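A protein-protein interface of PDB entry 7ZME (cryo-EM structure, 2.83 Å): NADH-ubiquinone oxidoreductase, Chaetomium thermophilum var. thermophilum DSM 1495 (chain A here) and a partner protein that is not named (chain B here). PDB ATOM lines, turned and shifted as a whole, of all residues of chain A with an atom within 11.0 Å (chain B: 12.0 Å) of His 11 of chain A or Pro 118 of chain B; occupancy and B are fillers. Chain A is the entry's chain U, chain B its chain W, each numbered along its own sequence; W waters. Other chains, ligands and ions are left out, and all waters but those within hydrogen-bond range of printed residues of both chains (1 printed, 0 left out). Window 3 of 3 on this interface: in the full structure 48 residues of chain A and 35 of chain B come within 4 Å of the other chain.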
ATOM      1  N   MET A   1      17.367 -13.214 -22.617  1.00  0.00           N
ATOM      2  CA  MET A   1      16.476 -12.077 -22.778  1.00  0.00           C
ATOM      3  C   MET A   1      16.243 -11.793 -24.257  1.00  0.00           C
ATOM      4  O   MET A   1      17.013 -12.236 -25.104  1.00  0.00           O
ATOM      5  CB  MET A   1      17.052 -10.863 -22.065  1.00  0.00           C
ATOM      6  N   ARG A   4      15.117  -8.201 -29.265  1.00  0.00           N
ATOM      7  CA  ARG A   4      14.650  -6.879 -29.730  1.00  0.00           C
ATOM      8  C   ARG A   4      15.648  -5.820 -29.277  1.00  0.00           C
ATOM      9  O   ARG A   4      16.176  -5.942 -28.162  1.00  0.00           O
ATOM     10  CB  ARG A   4      13.226  -6.590 -29.251  1.00  0.00           C
ATOM     11  CG  ARG A   4      13.032  -6.609 -27.744  1.00  0.00           C
ATOM     12  CD  ARG A   4      11.792  -5.818 -27.385  1.00  0.00           C
ATOM     13  NE  ARG A   4      11.750  -5.503 -25.967  1.00  0.00           N
ATOM     14  CZ  ARG A   4      12.291  -4.422 -25.421  1.00  0.00           C
ATOM     15  NH1 ARG A   4      12.196  -4.217 -24.120  1.00  0.00           N
ATOM     16  NH2 ARG A   4      12.931  -3.548 -26.177  1.00  0.00           N
ATOM     17  N   PRO A   6      16.549  -2.473 -27.634  1.00  0.00           N
ATOM     18  CA  PRO A   6      15.851  -1.592 -26.699  1.00  0.00           C
ATOM     19  C   PRO A   6      15.742  -0.130 -27.150  1.00  0.00           C
ATOM     20  O   PRO A   6      16.673   0.363 -27.754  1.00  0.00           O
ATOM     21  CB  PRO A   6      16.737  -1.678 -25.449  1.00  0.00           C
ATOM     22  CG  PRO A   6      18.099  -2.062 -25.963  1.00  0.00           C
ATOM     23  CD  PRO A   6      17.793  -3.017 -27.090  1.00  0.00           C
ATOM     24  N   ALA A   7      14.621   0.528 -26.851  1.00  0.00           N
ATOM     25  CA  ALA A   7      14.480   1.936 -27.178  1.00  0.00           C
ATOM     26  C   ALA A   7      14.447   2.839 -25.961  1.00  0.00           C
ATOM     27  O   ALA A   7      14.622   4.049 -26.106  1.00  0.00           O
ATOM     28  CB  ALA A   7      13.205   2.172 -28.003  1.00  0.00           C
ATOM     29  N   PHE A   8      14.231   2.285 -24.768  1.00  0.00           N
ATOM     30  CA  PHE A   8      14.130   3.066 -23.543  1.00  0.00           C
ATOM     31  C   PHE A   8      14.886   2.417 -22.390  1.00  0.00           C
ATOM     32  O   PHE A   8      14.461   2.519 -21.237  1.00  0.00           O
ATOM     33  CB  PHE A   8      12.661   3.276 -23.171  1.00  0.00           C
ATOM     34  CG  PHE A   8      11.898   4.091 -24.172  1.00  0.00           C
ATOM     35  CD1 PHE A   8      11.969   5.466 -24.166  1.00  0.00           C
ATOM     36  CD2 PHE A   8      11.121   3.476 -25.132  1.00  0.00           C
ATOM     37  CE1 PHE A   8      11.273   6.209 -25.089  1.00  0.00           C
ATOM     38  CE2 PHE A   8      10.426   4.213 -26.058  1.00  0.00           C
ATOM     39  CZ  PHE A   8      10.501   5.585 -26.035  1.00  0.00           C
ATOM     40  N   ASN A   9      15.992   1.742 -22.681  1.00  0.00           N
ATOM     41  CA  ASN A   9      16.770   1.088 -21.639  1.00  0.00           C
ATOM     42  C   ASN A   9      17.542   2.126 -20.832  1.00  0.00           C
ATOM     43  O   ASN A   9      18.221   2.986 -21.398  1.00  0.00           O
ATOM     44  CB  ASN A   9      17.727   0.073 -22.254  1.00  0.00           C
ATOM     45  CG  ASN A   9      18.563   0.665 -23.368  1.00  0.00           C
ATOM     46  OD1 ASN A   9      18.035   1.251 -24.310  1.00  0.00           O
ATOM     47  ND2 ASN A   9      19.874   0.514 -23.267  1.00  0.00           N
ATOM     48  N   GLN A  10      17.432   2.046 -19.511  1.00  0.00           N
ATOM     49  CA  GLN A  10      18.217   2.870 -18.610  1.00  0.00           C
ATOM     50  C   GLN A  10      18.928   2.044 -17.553  1.00  0.00           C
ATOM     51  O   GLN A  10      19.600   2.618 -16.691  1.00  0.00           O
ATOM     52  CB  GLN A  10      17.334   3.919 -17.919  1.00  0.00           C
ATOM     53  CG  GLN A  10      16.475   4.736 -18.861  1.00  0.00           C
ATOM     54  CD  GLN A  10      17.216   5.926 -19.431  1.00  0.00           C
ATOM     55  OE1 GLN A  10      17.409   6.030 -20.639  1.00  0.00           O
ATOM     56  NE2 GLN A  10      17.640   6.832 -18.557  1.00  0.00           N
ATOM     57  N   HIS A  11      18.786   0.724 -17.610  1.00  0.00           N
ATOM     58  CA  HIS A  11      19.326  -0.129 -16.526  1.00  0.00           C
ATOM     59  C   HIS A  11      19.854  -1.440 -17.065  1.00  0.00           C
ATOM     60  O   HIS A  11      19.380  -1.883 -18.108  1.00  0.00           O
ATOM     61  CB  HIS A  11      18.233  -0.448 -15.497  1.00  0.00           C
ATOM     62  CG  HIS A  11      17.782   0.731 -14.709  1.00  0.00           C
ATOM     63  ND1 HIS A  11      18.559   1.292 -13.719  1.00  0.00           N
ATOM     64  CD2 HIS A  11      16.648   1.459 -14.765  1.00  0.00           C
ATOM     65  CE1 HIS A  11      17.925   2.318 -13.196  1.00  0.00           C
ATOM     66  NE2 HIS A  11      16.749   2.442 -13.821  1.00  0.00           N
ATOM     67  N   VAL A  12      20.882  -1.961 -16.407  1.00  0.00           N
ATOM     68  CA  VAL A  12      21.463  -3.271 -16.795  1.00  0.00           C
ATOM     69  C   VAL A  12      21.236  -4.242 -15.632  1.00  0.00           C
ATOM     70  O   VAL A  12      21.425  -3.825 -14.481  1.00  0.00           O
ATOM     71  CB  VAL A  12      22.955  -3.095 -17.132  1.00  0.00           C
ATOM     72  CG1 VAL A  12      23.747  -4.375 -16.948  1.00  0.00           C
ATOM     73  CG2 VAL A  12      23.159  -2.513 -18.522  1.00  0.00           C
ATOM     74  N   LEU A  13      20.786  -5.464 -15.914  1.00  0.00           N
ATOM     75  CA  LEU A  13      20.627  -6.496 -14.858  1.00  0.00           C
ATOM     76  C   LEU A  13      21.757  -7.510 -15.033  1.00  0.00           C
ATOM     77  O   LEU A  13      21.985  -7.928 -16.173  1.00  0.00           O
ATOM     78  CB  LEU A  13      19.254  -7.157 -14.993  1.00  0.00           C
ATOM     79  CG  LEU A  13      18.810  -8.024 -13.818  1.00  0.00           C
ATOM     80  CD1 LEU A  13      18.760  -7.215 -12.531  1.00  0.00           C
ATOM     81  CD2 LEU A  13      17.456  -8.644 -14.108  1.00  0.00           C
ATOM     82  N   LEU A  14      22.455  -7.854 -13.949  1.00  0.00           N
ATOM     83  CA  LEU A  14      23.572  -8.828 -14.001  1.00  0.00           C
ATOM     84  C   LEU A  14      23.256  -9.999 -13.072  1.00  0.00           C
ATOM     85  O   LEU A  14      22.580  -9.774 -12.064  1.00  0.00           O
ATOM     86  CB  LEU A  14      24.872  -8.139 -13.573  1.00  0.00           C
ATOM     87  CG  LEU A  14      25.348  -6.989 -14.455  1.00  0.00           C
ATOM     88  CD1 LEU A  14      25.060  -5.651 -13.792  1.00  0.00           C
ATOM     89  CD2 LEU A  14      26.832  -7.117 -14.743  1.00  0.00           C
ATOM     90  N   ARG B  82      21.951 -18.022 -16.733  1.00  0.00           N
ATOM     91  CA  ARG B  82      20.884 -17.143 -16.182  1.00  0.00           C
ATOM     92  C   ARG B  82      19.559 -17.888 -16.073  1.00  0.00           C
ATOM     93  O   ARG B  82      18.810 -17.590 -15.137  1.00  0.00           O
ATOM     94  CB  ARG B  82      20.826 -15.787 -16.890  1.00  0.00           C
ATOM     95  CG  ARG B  82      22.113 -14.990 -16.757  1.00  0.00           C
ATOM     96  CD  ARG B  82      21.966 -13.528 -17.111  1.00  0.00           C
ATOM     97  NE  ARG B  82      21.089 -12.826 -16.193  1.00  0.00           N
ATOM     98  CZ  ARG B  82      21.010 -11.507 -16.095  1.00  0.00           C
ATOM     99  NH1 ARG B  82      20.180 -10.957 -15.228  1.00  0.00           N
ATOM    100  NH2 ARG B  82      21.769 -10.741 -16.853  1.00  0.00           N
ATOM    101  N   THR B 110      11.142 -12.320 -21.793  1.00  0.00           N
ATOM    102  CA  THR B 110      10.636 -10.959 -22.127  1.00  0.00           C
ATOM    103  C   THR B 110      10.675 -10.124 -20.853  1.00  0.00           C
ATOM    104  O   THR B 110      10.809  -8.902 -20.944  1.00  0.00           O
ATOM    105  CB  THR B 110       9.201 -11.065 -22.659  1.00  0.00           C
ATOM    106  OG1 THR B 110       9.247 -11.891 -23.818  1.00  0.00           O
ATOM    107  CG2 THR B 110       8.569  -9.736 -23.003  1.00  0.00           C
ATOM    108  N   PHE B 111      10.606 -10.795 -19.709  1.00  0.00           N
ATOM    109  CA  PHE B 111      10.525 -10.104 -18.407  1.00  0.00           C
ATOM    110  C   PHE B 111      11.557 -10.714 -17.468  1.00  0.00           C
ATOM    111  O   PHE B 111      11.808 -11.923 -17.567  1.00  0.00           O
ATOM    112  CB  PHE B 111       9.145 -10.357 -17.797  1.00  0.00           C
ATOM    113  CG  PHE B 111       7.970  -9.802 -18.556  1.00  0.00           C
ATOM    114  CD1 PHE B 111       7.697  -8.445 -18.545  1.00  0.00           C
ATOM    115  CD2 PHE B 111       7.121 -10.641 -19.257  1.00  0.00           C
ATOM    116  CE1 PHE B 111       6.605  -7.940 -19.230  1.00  0.00           C
ATOM    117  CE2 PHE B 111       6.036 -10.132 -19.949  1.00  0.00           C
ATOM    118  CZ  PHE B 111       5.779  -8.783 -19.932  1.00  0.00           C
ATOM    119  N   ALA B 112      12.113  -9.907 -16.570  1.00  0.00           N
ATOM    120  CA  ALA B 112      13.056 -10.453 -15.572  1.00  0.00           C
ATOM    121  C   ALA B 112      12.778  -9.865 -14.196  1.00  0.00           C
ATOM    122  O   ALA B 112      12.394  -8.694 -14.138  1.00  0.00           O
ATOM    123  CB  ALA B 112      14.474 -10.183 -15.983  1.00  0.00           C
ATOM    124  N   VAL B 113      12.936 -10.661 -13.145  1.00  0.00           N
ATOM    125  CA  VAL B 113      12.830 -10.164 -11.781  1.00  0.00           C
ATOM    126  C   VAL B 113      13.971  -9.190 -11.525  1.00  0.00           C
ATOM    127  O   VAL B 113      15.139  -9.493 -11.794  1.00  0.00           O
ATOM    128  CB  VAL B 113      12.856 -11.331 -10.783  1.00  0.00           C
ATOM    129  CG1 VAL B 113      13.269 -10.849  -9.403  1.00  0.00           C
ATOM    130  CG2 VAL B 113      11.516 -12.022 -10.731  1.00  0.00           C
ATOM    131  N   THR B 114      13.642  -8.010 -11.015  1.00  0.00           N
ATOM    132  CA  THR B 114      14.667  -7.031 -10.696  1.00  0.00           C
ATOM    133  C   THR B 114      14.541  -6.609  -9.241  1.00  0.00           C
ATOM    134  O   THR B 114      13.449  -6.659  -8.666  1.00  0.00           O
ATOM    135  CB  THR B 114      14.574  -5.788 -11.598  1.00  0.00           C
ATOM    136  OG1 THR B 114      13.526  -4.930 -11.135  1.00  0.00           O
ATOM    137  CG2 THR B 114      14.312  -6.179 -13.043  1.00  0.00           C
ATOM    138  N   PRO B 115      15.643  -6.202  -8.619  1.00  0.00           N
ATOM    139  CA  PRO B 115      15.570  -5.698  -7.246  1.00  0.00           C
ATOM    140  C   PRO B 115      14.865  -4.353  -7.183  1.00  0.00           C
ATOM    141  O   PRO B 115      14.726  -3.638  -8.177  1.00  0.00           O
ATOM    142  CB  PRO B 115      17.039  -5.574  -6.830  1.00  0.00           C
ATOM    143  CG  PRO B 115      17.802  -5.546  -8.102  1.00  0.00           C
ATOM    144  CD  PRO B 115      17.031  -6.355  -9.080  1.00  0.00           C
ATOM    145  N   SER B 116      14.416  -4.013  -5.978  1.00  0.00           N
ATOM    146  CA  SER B 116      13.634  -2.802  -5.776  1.00  0.00           C
ATOM    147  C   SER B 116      14.464  -1.531  -5.856  1.00  0.00           C
ATOM    148  O   SER B 116      13.889  -0.437  -5.886  1.00  0.00           O
ATOM    149  CB  SER B 116      12.921  -2.859  -4.425  1.00  0.00           C
ATOM    150  OG  SER B 116      12.419  -1.585  -4.061  1.00  0.00           O
ATOM    151  N   LYS B 117      15.791  -1.639  -5.891  1.00  0.00           N
ATOM    152  CA  LYS B 117      16.652  -0.474  -5.948  1.00  0.00           C
ATOM    153  C   LYS B 117      17.828  -0.742  -6.875  1.00  0.00           C
ATOM    154  O   LYS B 117      18.351  -1.864  -6.903  1.00  0.00           O
ATOM    155  CB  LYS B 117      17.169  -0.108  -4.549  1.00  0.00           C
ATOM    156  CG  LYS B 117      17.828   1.257  -4.455  1.00  0.00           C
ATOM    157  CD  LYS B 117      18.256   1.563  -3.028  1.00  0.00           C
ATOM    158  CE  LYS B 117      17.080   2.026  -2.184  1.00  0.00           C
ATOM    159  NZ  LYS B 117      17.526   2.707  -0.939  1.00  0.00           N
ATOM    160  N   PRO B 118      18.261   0.257  -7.644  1.00  0.00           N
ATOM    161  CA  PRO B 118      19.530   0.127  -8.371  1.00  0.00           C
ATOM    162  C   PRO B 118      20.716   0.253  -7.431  1.00  0.00           C
ATOM    163  O   PRO B 118      20.538   0.400  -6.219  1.00  0.00           O
ATOM    164  CB  PRO B 118      19.485   1.282  -9.380  1.00  0.00           C
ATOM    165  CG  PRO B 118      18.060   1.731  -9.409  1.00  0.00           C
ATOM    166  CD  PRO B 118      17.518   1.459  -8.047  1.00  0.00           C
ATOM    167  N   ALA B 119      21.928   0.194  -7.972  1.00  0.00           N
ATOM    168  CA  ALA B 119      23.110   0.361  -7.139  1.00  0.00           C
ATOM    169  C   ALA B 119      23.158   1.774  -6.568  1.00  0.00           C
ATOM    170  O   ALA B 119      22.768   2.742  -7.225  1.00  0.00           O
ATOM    171  CB  ALA B 119      24.371   0.063  -7.944  1.00  0.00           C
ATOM    172  N   GLN B 120      23.642   1.886  -5.328  1.00  0.00           N
ATOM    173  CA  GLN B 120      23.576   3.155  -4.610  1.00  0.00           C
ATOM    174  C   GLN B 120      24.455   4.235  -5.228  1.00  0.00           C
ATOM    175  O   GLN B 120      24.134   5.421  -5.093  1.00  0.00           O
ATOM    176  CB  GLN B 120      23.966   2.948  -3.146  1.00  0.00           C
ATOM    177  CG  GLN B 120      23.515   4.067  -2.220  1.00  0.00           C
ATOM    178  CD  GLN B 120      22.101   4.537  -2.511  1.00  0.00           C
ATOM    179  OE1 GLN B 120      21.169   3.736  -2.581  1.00  0.00           O
ATOM    180  NE2 GLN B 120      21.938   5.844  -2.685  1.00  0.00           N
ATOM    181  N   GLU B 121      25.542   3.857  -5.895  1.00  0.00           N
ATOM    182  CA  GLU B 121      26.468   4.813  -6.504  1.00  0.00           C
ATOM    183  C   GLU B 121      27.012   5.807  -5.484  1.00  0.00           C
ATOM    184  O   GLU B 121      28.129   6.305  -5.623  1.00  0.00           O
ATOM    185  CB  GLU B 121      25.791   5.562  -7.657  1.00  0.00           C
HETATM  186  O   HOH W   1      11.597  -7.977 -23.960  1.00  0.00           O
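Of the 11 printed residues of chain A, 3 touch a printed residue of chain B. Printed residues of chain A that touch a printed residue of chain B: His 11, Leu 13 and Leu 14. Hydrophobic or aromatic side chains of chain A that line the printed part of chain B: His 11 and Leu 13. Along chain A the printed residues that touch a printed residue of chain B span positions 11 to 14. Among the printed residues, 6 pairs touch across the chains. Among the printed residues, no Asp or Glu carboxylate lies within 4 Å of a Lys or Arg side-chain nitrogen of the other chain.
The backbone carbonyl oxygen (O) of Leu 13 of chain A sits at hydrogen-bond distance from the guanidinium group (NH2) of Arg 82 of chain B.
Pro 118 of chain B touches His 11 of chain A (CG to CE1, 3.8 Å). Ala 112 of chain B touches Leu 13 of chain A (CB to CD2, 3.8 Å). CD2 of Leu 13 of chain A touches O of Val 113 of chain B, 3.4 Å away. CD1 of Leu 13 of chain A touches CD of Pro 115 of chain B, 3.95 Å away. Leu 14 of chain A touches Arg 82 of chain B.
Of the printed residues of chain A, Pro 118 of chain B touches His 11 (3.8 Å). No residue of chain B comes within 4 Å of Asn 9 of chain A. No residue of chain B comes within 4 Å of Val 12 of chain A. No residue of chain A comes within 4 Å of Lys 117 of chain B. No residue of chain A comes within 4 Å of Ala 119 of chain B. Printed residues of chain B within 4 Å of Leu 13 of chain A: Arg 82, Ala 112, Val 113 and Pro 115. Of the printed residues of chain A, Ala 112 of chain B touches Leu 13 (3.8 Å). Of the printed residues of chain A, Arg 82 of chain B touches Leu 13 and Leu 14. Of the printed residues of chain B, Leu 14 of chain A touches Arg 82 (3.9 Å). Of the printed residues of chain A, Val 113 of chain B touches Leu 13 (3.4 Å).
Water W1 lies within hydrogen-bond range of NE of Arg 4 of chain A and O of Thr 110 of chain B.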
